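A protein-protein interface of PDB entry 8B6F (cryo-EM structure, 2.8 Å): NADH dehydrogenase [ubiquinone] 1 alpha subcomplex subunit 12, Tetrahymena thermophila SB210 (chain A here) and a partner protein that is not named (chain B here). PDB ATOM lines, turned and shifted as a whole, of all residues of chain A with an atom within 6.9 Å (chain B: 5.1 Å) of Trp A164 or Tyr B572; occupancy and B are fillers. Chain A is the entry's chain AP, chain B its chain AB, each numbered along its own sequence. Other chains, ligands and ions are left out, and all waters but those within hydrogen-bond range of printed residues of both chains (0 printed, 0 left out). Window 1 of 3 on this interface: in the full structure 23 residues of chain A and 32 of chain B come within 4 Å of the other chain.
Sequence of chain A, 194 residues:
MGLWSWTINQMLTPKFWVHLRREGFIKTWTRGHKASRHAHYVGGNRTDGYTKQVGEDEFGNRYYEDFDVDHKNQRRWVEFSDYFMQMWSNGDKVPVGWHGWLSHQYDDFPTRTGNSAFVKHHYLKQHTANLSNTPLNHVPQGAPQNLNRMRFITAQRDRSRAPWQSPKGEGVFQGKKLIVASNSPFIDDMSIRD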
ATOM      1  N   ALA A 162     -32.991  26.816  26.614  1.00  0.00           N
ATOM      2  CA  ALA A 162     -32.245  27.408  25.514  1.00  0.00           C
ATOM      3  C   ALA A 162     -32.209  26.433  24.349  1.00  0.00           C
ATOM      4  O   ALA A 162     -31.697  25.316  24.515  1.00  0.00           O
ATOM      5  CB  ALA A 162     -30.829  27.763  25.950  1.00  0.00           C
ATOM      6  N   PRO A 163     -32.732  26.784  23.174  1.00  0.00           N
ATOM      7  CA  PRO A 163     -32.701  25.840  22.052  1.00  0.00           C
ATOM      8  C   PRO A 163     -31.278  25.465  21.669  1.00  0.00           C
ATOM      9  O   PRO A 163     -30.346  26.263  21.794  1.00  0.00           O
ATOM     10  CB  PRO A 163     -33.399  26.605  20.922  1.00  0.00           C
ATOM     11  CG  PRO A 163     -34.213  27.641  21.602  1.00  0.00           C
ATOM     12  CD  PRO A 163     -33.442  28.026  22.822  1.00  0.00           C
ATOM     13  N   TRP A 164     -31.116  24.226  21.209  1.00  0.00           N
ATOM     14  CA  TRP A 164     -29.825  23.760  20.722  1.00  0.00           C
ATOM     15  C   TRP A 164     -29.553  24.334  19.339  1.00  0.00           C
ATOM     16  O   TRP A 164     -30.394  24.235  18.440  1.00  0.00           O
ATOM     17  CB  TRP A 164     -29.802  22.233  20.678  1.00  0.00           C
ATOM     18  CG  TRP A 164     -28.621  21.658  19.961  1.00  0.00           C
ATOM     19  CD1 TRP A 164     -27.311  21.772  20.317  1.00  0.00           C
ATOM     20  CD2 TRP A 164     -28.647  20.859  18.771  1.00  0.00           C
ATOM     21  NE1 TRP A 164     -26.516  21.101  19.418  1.00  0.00           N
ATOM     22  CE2 TRP A 164     -27.312  20.532  18.459  1.00  0.00           C
ATOM     23  CE3 TRP A 164     -29.668  20.393  17.937  1.00  0.00           C
ATOM     24  CZ2 TRP A 164     -26.971  19.761  17.350  1.00  0.00           C
ATOM     25  CZ3 TRP A 164     -29.328  19.625  16.834  1.00  0.00           C
ATOM     26  CH2 TRP A 164     -27.990  19.318  16.552  1.00  0.00           C
ATOM     27  N   GLN A 165     -28.377  24.935  19.167  1.00  0.00           N
ATOM     28  CA  GLN A 165     -28.014  25.553  17.894  1.00  0.00           C
ATOM     29  C   GLN A 165     -27.539  24.464  16.943  1.00  0.00           C
ATOM     30  O   GLN A 165     -26.417  23.968  17.057  1.00  0.00           O
ATOM     31  CB  GLN A 165     -26.935  26.608  18.103  1.00  0.00           C
ATOM     32  CG  GLN A 165     -27.321  27.721  19.070  1.00  0.00           C
ATOM     33  CD  GLN A 165     -28.493  28.554  18.581  1.00  0.00           C
ATOM     34  OE1 GLN A 165     -29.596  28.046  18.381  1.00  0.00           O
ATOM     35  NE2 GLN A 165     -28.255  29.848  18.388  1.00  0.00           N
ATOM     36  N   SER A 166     -28.391  24.089  16.008  1.00  0.00           N
ATOM     37  CA  SER A 166     -28.065  23.023  15.079  1.00  0.00           C
ATOM     38  C   SER A 166     -27.097  23.513  14.002  1.00  0.00           C
ATOM     39  O   SER A 166     -27.099  24.693  13.646  1.00  0.00           O
ATOM     40  CB  SER A 166     -29.327  22.455  14.453  1.00  0.00           C
ATOM     41  OG  SER A 166     -30.182  22.011  15.491  1.00  0.00           O
ATOM     42  N   PRO A 167     -26.259  22.625  13.469  1.00  0.00           N
ATOM     43  CA  PRO A 167     -25.358  23.032  12.385  1.00  0.00           C
ATOM     44  C   PRO A 167     -26.129  23.511  11.165  1.00  0.00           C
ATOM     45  O   PRO A 167     -27.224  23.034  10.862  1.00  0.00           O
ATOM     46  CB  PRO A 167     -24.572  21.752  12.076  1.00  0.00           C
ATOM     47  CG  PRO A 167     -24.651  20.948  13.321  1.00  0.00           C
ATOM     48  CD  PRO A 167     -25.989  21.249  13.918  1.00  0.00           C
ATOM     49  N   PHE A 173     -18.191  15.490   7.636  1.00  0.00           N
ATOM     50  CA  PHE A 173     -18.878  14.251   7.973  1.00  0.00           C
ATOM     51  C   PHE A 173     -17.857  13.153   8.224  1.00  0.00           C
ATOM     52  O   PHE A 173     -16.921  12.978   7.436  1.00  0.00           O
ATOM     53  CB  PHE A 173     -19.833  13.826   6.855  1.00  0.00           C
ATOM     54  CG  PHE A 173     -21.171  14.502   6.910  1.00  0.00           C
ATOM     55  CD1 PHE A 173     -21.368  15.730   6.304  1.00  0.00           C
ATOM     56  CD2 PHE A 173     -22.235  13.902   7.561  1.00  0.00           C
ATOM     57  CE1 PHE A 173     -22.600  16.351   6.353  1.00  0.00           C
ATOM     58  CE2 PHE A 173     -23.469  14.516   7.613  1.00  0.00           C
ATOM     59  CZ  PHE A 173     -23.652  15.741   7.009  1.00  0.00           C
ATOM     60  N   LYS A 176     -21.629   8.483   9.334  1.00  0.00           N
ATOM     61  CA  LYS A 176     -22.906   9.132   9.623  1.00  0.00           C
ATOM     62  C   LYS A 176     -22.791   9.915  10.929  1.00  0.00           C
ATOM     63  O   LYS A 176     -23.380   9.579  11.956  1.00  0.00           O
ATOM     64  CB  LYS A 176     -24.027   8.101   9.683  1.00  0.00           C
ATOM     65  CG  LYS A 176     -24.554   7.692   8.319  1.00  0.00           C
ATOM     66  CD  LYS A 176     -25.992   7.208   8.392  1.00  0.00           C
ATOM     67  CE  LYS A 176     -26.974   8.352   8.615  1.00  0.00           C
ATOM     68  NZ  LYS A 176     -26.931   9.358   7.516  1.00  0.00           N
ATOM     69  N   LYS A 177     -21.999  10.981  10.867  1.00  0.00           N
ATOM     70  CA  LYS A 177     -21.830  11.872  12.003  1.00  0.00           C
ATOM     71  C   LYS A 177     -21.317  13.208  11.494  1.00  0.00           C
ATOM     72  O   LYS A 177     -20.451  13.250  10.617  1.00  0.00           O
ATOM     73  CB  LYS A 177     -20.860  11.295  13.038  1.00  0.00           C
ATOM     74  CG  LYS A 177     -20.791  12.102  14.327  1.00  0.00           C
ATOM     75  CD  LYS A 177     -19.645  11.645  15.212  1.00  0.00           C
ATOM     76  CE  LYS A 177     -19.695  12.322  16.574  1.00  0.00           C
ATOM     77  NZ  LYS A 177     -19.650  13.808  16.470  1.00  0.00           N
ATOM     78  N   LEU A 178     -21.851  14.289  12.049  1.00  0.00           N
ATOM     79  CA  LEU A 178     -21.419  15.639  11.721  1.00  0.00           C
ATOM     80  C   LEU A 178     -20.466  16.112  12.811  1.00  0.00           C
ATOM     81  O   LEU A 178     -20.825  16.116  13.994  1.00  0.00           O
ATOM     82  CB  LEU A 178     -22.618  16.578  11.596  1.00  0.00           C
ATOM     83  CG  LEU A 178     -22.472  17.726  10.594  1.00  0.00           C
ATOM     84  CD1 LEU A 178     -23.775  18.497  10.484  1.00  0.00           C
ATOM     85  CD2 LEU A 178     -21.334  18.654  10.977  1.00  0.00           C
ATOM     86  N   ILE A 179     -19.259  16.500  12.416  1.00  0.00           N
ATOM     87  CA  ILE A 179     -18.213  16.876  13.359  1.00  0.00           C
ATOM     88  C   ILE A 179     -18.278  18.381  13.583  1.00  0.00           C
ATOM     89  O   ILE A 179     -18.115  19.165  12.642  1.00  0.00           O
ATOM     90  CB  ILE A 179     -16.828  16.455  12.846  1.00  0.00           C
ATOM     91  CG1 ILE A 179     -16.815  14.964  12.494  1.00  0.00           C
ATOM     92  CG2 ILE A 179     -15.756  16.770  13.881  1.00  0.00           C
ATOM     93  CD1 ILE A 179     -17.192  14.046  13.641  1.00  0.00           C
ATOM     94  N   VAL A 180     -18.513  18.783  14.829  1.00  0.00           N
ATOM     95  CA  VAL A 180     -18.578  20.190  15.209  1.00  0.00           C
ATOM     96  C   VAL A 180     -17.788  20.379  16.495  1.00  0.00           C
ATOM     97  O   VAL A 180     -17.859  19.551  17.408  1.00  0.00           O
ATOM     98  CB  VAL A 180     -20.035  20.669  15.385  1.00  0.00           C
ATOM     99  CG1 VAL A 180     -20.831  20.416  14.120  1.00  0.00           C
ATOM    100  CG2 VAL A 180     -20.694  19.980  16.576  1.00  0.00           C
ATOM    101  N   ALA A 181     -17.027  21.467  16.561  1.00  0.00           N
ATOM    102  CA  ALA A 181     -16.278  21.778  17.768  1.00  0.00           C
ATOM    103  C   ALA A 181     -17.226  22.124  18.910  1.00  0.00           C
ATOM    104  O   ALA A 181     -18.298  22.698  18.707  1.00  0.00           O
ATOM    105  CB  ALA A 181     -15.318  22.941  17.516  1.00  0.00           C
ATOM    106  N   ASN A 183     -18.928  24.006  21.867  1.00  0.00           N
ATOM    107  CA  ASN A 183     -19.178  25.418  22.123  1.00  0.00           C
ATOM    108  C   ASN A 183     -19.098  25.777  23.601  1.00  0.00           C
ATOM    109  O   ASN A 183     -19.381  26.924  23.960  1.00  0.00           O
ATOM    110  CB  ASN A 183     -20.552  25.817  21.577  1.00  0.00           C
ATOM    111  CG  ASN A 183     -21.688  25.110  22.291  1.00  0.00           C
ATOM    112  OD1 ASN A 183     -22.124  24.036  21.877  1.00  0.00           O
ATOM    113  ND2 ASN A 183     -22.175  25.712  23.371  1.00  0.00           N
ATOM    114  N   GLN B 301     -29.571  23.567  25.471  1.00  0.00           N
ATOM    115  CA  GLN B 301     -29.279  22.529  24.484  1.00  0.00           C
ATOM    116  C   GLN B 301     -30.435  21.538  24.391  1.00  0.00           C
ATOM    117  O   GLN B 301     -30.242  20.322  24.354  1.00  0.00           O
ATOM    118  CB  GLN B 301     -27.969  21.813  24.811  1.00  0.00           C
ATOM    119  CG  GLN B 301     -26.737  22.669  24.590  1.00  0.00           C
ATOM    120  CD  GLN B 301     -25.453  21.887  24.754  1.00  0.00           C
ATOM    121  OE1 GLN B 301     -25.437  20.818  25.361  1.00  0.00           O
ATOM    122  NE2 GLN B 301     -24.366  22.416  24.207  1.00  0.00           N
ATOM    123  N   ARG B 302     -31.648  22.076  24.343  1.00  0.00           N
ATOM    124  CA  ARG B 302     -32.866  21.280  24.284  1.00  0.00           C
ATOM    125  C   ARG B 302     -33.425  21.308  22.869  1.00  0.00           C
ATOM    126  O   ARG B 302     -33.552  22.379  22.267  1.00  0.00           O
ATOM    127  CB  ARG B 302     -33.909  21.808  25.270  1.00  0.00           C
ATOM    128  CG  ARG B 302     -33.509  21.695  26.735  1.00  0.00           C
ATOM    129  CD  ARG B 302     -33.340  20.249  27.166  1.00  0.00           C
ATOM    130  NE  ARG B 302     -34.531  19.451  26.896  1.00  0.00           N
ATOM    131  CZ  ARG B 302     -35.558  19.322  27.724  1.00  0.00           C
ATOM    132  NH1 ARG B 302     -35.584  19.933  28.896  1.00  0.00           N
ATOM    133  NH2 ARG B 302     -36.586  18.558  27.368  1.00  0.00           N
ATOM    134  N   ILE B 303     -33.749  20.132  22.342  1.00  0.00           N
ATOM    135  CA  ILE B 303     -34.391  20.026  21.038  1.00  0.00           C
ATOM    136  C   ILE B 303     -35.871  20.339  21.217  1.00  0.00           C
ATOM    137  O   ILE B 303     -36.552  19.710  22.034  1.00  0.00           O
ATOM    138  CB  ILE B 303     -34.187  18.630  20.435  1.00  0.00           C
ATOM    139  CG1 ILE B 303     -32.695  18.307  20.325  1.00  0.00           C
ATOM    140  CG2 ILE B 303     -34.839  18.540  19.064  1.00  0.00           C
ATOM    141  CD1 ILE B 303     -32.405  16.835  20.165  1.00  0.00           C
ATOM    142  N   MET B 307     -36.578  17.902  13.291  1.00  0.00           N
ATOM    143  CA  MET B 307     -35.572  18.429  12.381  1.00  0.00           C
ATOM    144  C   MET B 307     -35.155  17.353  11.391  1.00  0.00           C
ATOM    145  O   MET B 307     -35.270  16.156  11.666  1.00  0.00           O
ATOM    146  CB  MET B 307     -34.344  18.954  13.131  1.00  0.00           C
ATOM    147  CG  MET B 307     -34.694  19.757  14.374  1.00  0.00           C
ATOM    148  SD  MET B 307     -33.268  20.560  15.123  1.00  0.00           S
ATOM    149  CE  MET B 307     -32.914  21.767  13.844  1.00  0.00           C
ATOM    150  N   ARG B 309     -31.862  16.600   8.455  1.00  0.00           N
ATOM    151  CA  ARG B 309     -30.524  16.977   8.022  1.00  0.00           C
ATOM    152  C   ARG B 309     -30.354  16.650   6.546  1.00  0.00           C
ATOM    153  O   ARG B 309     -30.655  15.532   6.115  1.00  0.00           O
ATOM    154  CB  ARG B 309     -29.461  16.252   8.850  1.00  0.00           C
ATOM    155  CG  ARG B 309     -28.032  16.633   8.498  1.00  0.00           C
ATOM    156  CD  ARG B 309     -27.025  15.804   9.281  1.00  0.00           C
ATOM    157  NE  ARG B 309     -27.124  14.385   8.960  1.00  0.00           N
ATOM    158  CZ  ARG B 309     -26.356  13.440   9.485  1.00  0.00           C
ATOM    159  NH1 ARG B 309     -25.411  13.726  10.364  1.00  0.00           N
ATOM    160  NH2 ARG B 309     -26.541  12.176   9.118  1.00  0.00           N
ATOM    161  N   TYR B 315     -29.202  21.305   9.010  1.00  0.00           N
ATOM    162  CA  TYR B 315     -30.429  20.968   9.717  1.00  0.00           C
ATOM    163  C   TYR B 315     -31.515  21.998   9.429  1.00  0.00           C
ATOM    164  O   TYR B 315     -31.245  23.198   9.330  1.00  0.00           O
ATOM    165  CB  TYR B 315     -30.170  20.888  11.220  1.00  0.00           C
ATOM    166  CG  TYR B 315     -29.455  19.631  11.654  1.00  0.00           C
ATOM    167  CD1 TYR B 315     -28.082  19.503  11.509  1.00  0.00           C
ATOM    168  CD2 TYR B 315     -30.156  18.576  12.218  1.00  0.00           C
ATOM    169  CE1 TYR B 315     -27.427  18.355  11.911  1.00  0.00           C
ATOM    170  CE2 TYR B 315     -29.512  17.426  12.622  1.00  0.00           C
ATOM    171  CZ  TYR B 315     -28.148  17.321  12.467  1.00  0.00           C
ATOM    172  OH  TYR B 315     -27.507  16.174  12.870  1.00  0.00           O
ATOM    173  N   GLY B 567     -28.879  17.767  22.153  1.00  0.00           N
ATOM    174  CA  GLY B 567     -28.107  17.635  20.937  1.00  0.00           C
ATOM    175  C   GLY B 567     -26.620  17.425  21.125  1.00  0.00           C
ATOM    176  O   GLY B 567     -25.866  17.580  20.157  1.00  0.00           O
ATOM    177  N   ASP B 568     -26.167  17.078  22.331  1.00  0.00           N
ATOM    178  CA  ASP B 568     -24.736  16.878  22.545  1.00  0.00           C
ATOM    179  C   ASP B 568     -24.211  15.718  21.706  1.00  0.00           C
ATOM    180  O   ASP B 568     -23.153  15.827  21.076  1.00  0.00           O
ATOM    181  CB  ASP B 568     -24.455  16.634  24.028  1.00  0.00           C
ATOM    182  CG  ASP B 568     -25.128  15.381  24.553  1.00  0.00           C
ATOM    183  OD1 ASP B 568     -26.256  15.082  24.108  1.00  0.00           O
ATOM    184  OD2 ASP B 568     -24.528  14.693  25.404  1.00  0.00           O
ATOM    185  N   GLU B 569     -24.937  14.604  21.683  1.00  0.00           N
ATOM    186  CA  GLU B 569     -24.532  13.429  20.925  1.00  0.00           C
ATOM    187  C   GLU B 569     -25.786  12.704  20.466  1.00  0.00           C
ATOM    188  O   GLU B 569     -26.861  12.853  21.051  1.00  0.00           O
ATOM    189  CB  GLU B 569     -23.644  12.501  21.763  1.00  0.00           C
ATOM    190  CG  GLU B 569     -22.879  11.459  20.960  1.00  0.00           C
ATOM    191  CD  GLU B 569     -21.786  12.067  20.100  1.00  0.00           C
ATOM    192  OE1 GLU B 569     -21.611  13.303  20.146  1.00  0.00           O
ATOM    193  OE2 GLU B 569     -21.100  11.309  19.382  1.00  0.00           O
ATOM    194  N   GLY B 570     -25.639  11.913  19.405  1.00  0.00           N
ATOM    195  CA  GLY B 570     -26.763  11.237  18.800  1.00  0.00           C
ATOM    196  C   GLY B 570     -27.611  12.105  17.900  1.00  0.00           C
ATOM    197  O   GLY B 570     -28.292  11.574  17.015  1.00  0.00           O
ATOM    198  N   ALA B 571     -27.600  13.423  18.098  1.00  0.00           N
ATOM    199  CA  ALA B 571     -28.266  14.342  17.188  1.00  0.00           C
ATOM    200  C   ALA B 571     -27.435  14.637  15.948  1.00  0.00           C
ATOM    201  O   ALA B 571     -27.955  15.236  15.002  1.00  0.00           O
ATOM    202  CB  ALA B 571     -28.592  15.651  17.909  1.00  0.00           C
ATOM    203  N   TYR B 572     -26.164  14.241  15.934  1.00  0.00           N
ATOM    204  CA  TYR B 572     -25.327  14.399  14.755  1.00  0.00           C
ATOM    205  C   TYR B 572     -25.306  13.156  13.880  1.00  0.00           C
ATOM    206  O   TYR B 572     -24.949  13.250  12.701  1.00  0.00           O
ATOM    207  CB  TYR B 572     -23.898  14.758  15.173  1.00  0.00           C
ATOM    208  CG  TYR B 572     -23.811  16.035  15.975  1.00  0.00           C
ATOM    209  CD1 TYR B 572     -23.828  17.273  15.347  1.00  0.00           C
ATOM    210  CD2 TYR B 572     -23.717  16.004  17.359  1.00  0.00           C
ATOM    211  CE1 TYR B 572     -23.753  18.443  16.074  1.00  0.00           C
ATOM    212  CE2 TYR B 572     -23.641  17.169  18.096  1.00  0.00           C
ATOM    213  CZ  TYR B 572     -23.659  18.386  17.447  1.00  0.00           C
ATOM    214  OH  TYR B 572     -23.584  19.548  18.177  1.00  0.00           O
ATOM    215  N   TYR B 573     -25.678  12.001  14.426  1.00  0.00           N
ATOM    216  CA  TYR B 573     -25.837  10.782  13.649  1.00  0.00           C
ATOM    217  C   TYR B 573     -27.226  10.651  13.043  1.00  0.00           C
ATOM    218  O   TYR B 573     -27.478   9.691  12.309  1.00  0.00           O
ATOM    219  CB  TYR B 573     -25.564   9.550  14.520  1.00  0.00           C
ATOM    220  CG  TYR B 573     -24.257   9.577  15.277  1.00  0.00           C
ATOM    221  CD1 TYR B 573     -24.137  10.283  16.467  1.00  0.00           C
ATOM    222  CD2 TYR B 573     -23.155   8.868  14.823  1.00  0.00           C
ATOM    223  CE1 TYR B 573     -22.950  10.301  17.170  1.00  0.00           C
ATOM    224  CE2 TYR B 573     -21.962   8.880  15.518  1.00  0.00           C
ATOM    225  CZ  TYR B 573     -21.868   9.597  16.692  1.00  0.00           C
ATOM    226  OH  TYR B 573     -20.685   9.613  17.392  1.00  0.00           O
ATOM    227  N   ALA B 574     -28.126  11.584  13.331  1.00  0.00           N
ATOM    228  CA  ALA B 574     -29.542  11.432  13.027  1.00  0.00           C
ATOM    229  C   ALA B 574     -29.878  12.082  11.693  1.00  0.00           C
ATOM    230  O   ALA B 574     -29.563  13.255  11.471  1.00  0.00           O
ATOM    231  CB  ALA B 574     -30.400  12.045  14.135  1.00  0.00           C
ATOM    232  N   ILE B 577     -34.573  14.005  13.629  1.00  0.00           N
ATOM    233  CA  ILE B 577     -34.511  14.198  15.072  1.00  0.00           C
ATOM    234  C   ILE B 577     -35.914  14.509  15.570  1.00  0.00           C
ATOM    235  O   ILE B 577     -36.613  15.346  14.988  1.00  0.00           O
ATOM    236  CB  ILE B 577     -33.535  15.325  15.453  1.00  0.00           C
ATOM    237  CG1 ILE B 577     -32.130  14.987  14.949  1.00  0.00           C
ATOM    238  CG2 ILE B 577     -33.536  15.534  16.960  1.00  0.00           C
ATOM    239  CD1 ILE B 577     -31.099  16.056  15.227  1.00  0.00           C
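The backbone NH (N) of Gln B301 sits at hydrogen-bond distance from the backbone carbonyl oxygen (O) of Ala A162 (2.9 Å).
The backbone NH of Arg B302 lies within hydrogen-bond range of the backbone carbonyl oxygen of Ala A162, at 3.2 Å.
The backbone carbonyl oxygen (O) of Arg B302 is in hydrogen-bond range of the backbone NH (N) of Trp A164.
The side-chain hydroxyl (OG) of Ser A166 sits close to the side-chain sulfur (SD) of Met B307 (3.4 Å).
N of Tyr B315 lies within hydrogen-bond range of O of Pro A167 (3.2 Å).
O of Tyr B572 sits at hydrogen-bond distance from N of Leu A178, 3.3 Å away.
The side-chain amino group (NZ) of Lys A176 sits close to the guanidinium group (NH2) of Arg B309 (3.3 Å).
The backbone NH (N) of Ile B577 lies within hydrogen-bond range of the backbone carbonyl oxygen (O) of Met B307 (3.0 Å).
NH1 of Arg B309 sits at hydrogen-bond distance from O of Tyr B572 (2.4 Å).
OH of Tyr B573 lies within hydrogen-bond range of OE2 of Glu B569 (2.6 Å).
Among the printed residues, pairs that only touch across the chains: Lys A176 with Tyr B573, Lys A177 with Tyr B573, Lys A177 with Glu B569, Val A180 with Tyr B572, Phe A173 with Arg B309, Lys A177 with Tyr B572, Trp A164 with Tyr B572, Pro A163 with Arg B302, Asn A183 with Gln B301, Trp A164 with Gly B567, Ser A166 with Tyr B315, Pro A167 with Tyr B572, Trp A164 with Gln B301, Leu A178 with Tyr B315, Trp A164 with Ala B571 and Leu A178 with Arg B309.
Of the printed residues of chain B, Trp A164 touches Gln B301 (3.8 Å), Arg B302 (3.2 Å), Gly B567 (3.7 Å), Ala B571 (3.96 Å) and Tyr B572 (3.5 Å).
Of the printed residues of chain B, Ser A166 touches Met B307 and Tyr B315.
Of the printed residues of chain B, Lys A177 touches Glu B569 (3.3 Å), Tyr B572 (3.5 Å) and Tyr B573 (3.0 Å).
Of the printed residues of chain A, Glu B569 touches Lys A177 (3.3 Å).
Printed residues of chain A within 4 Å of Ala B571: Trp A164.
Of chain A, only Trp A164 (3.5 Å), Pro A167 (3.8 Å), Lys A177 (3.5 Å), Leu A178 (3.3 Å) and Val A180 (3.3 Å) come within 4 Å of Tyr B572.
Printed residues of chain A that touch a printed residue of chain B: Ala A162, Pro A163, Trp A164, Ser A166, Pro A167, Phe A173, Lys A176, Lys A177, Leu A178, Val A180 and Asn A183.
Hydrophobic or aromatic side chains of chain A within 4 Å of the printed part of chain B: Trp A164, Pro A167, Phe A173, Leu A178 and Val A180.
Of the 15 printed residues of chain B, 10 touch a printed residue of chain A.
Printed residues of chain B that touch a printed residue of chain A: Gln B301, Arg B302, Met B307, Arg B309, Tyr B315, Gly B567, Glu B569, Ala B571, Tyr B572 and Tyr B573.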
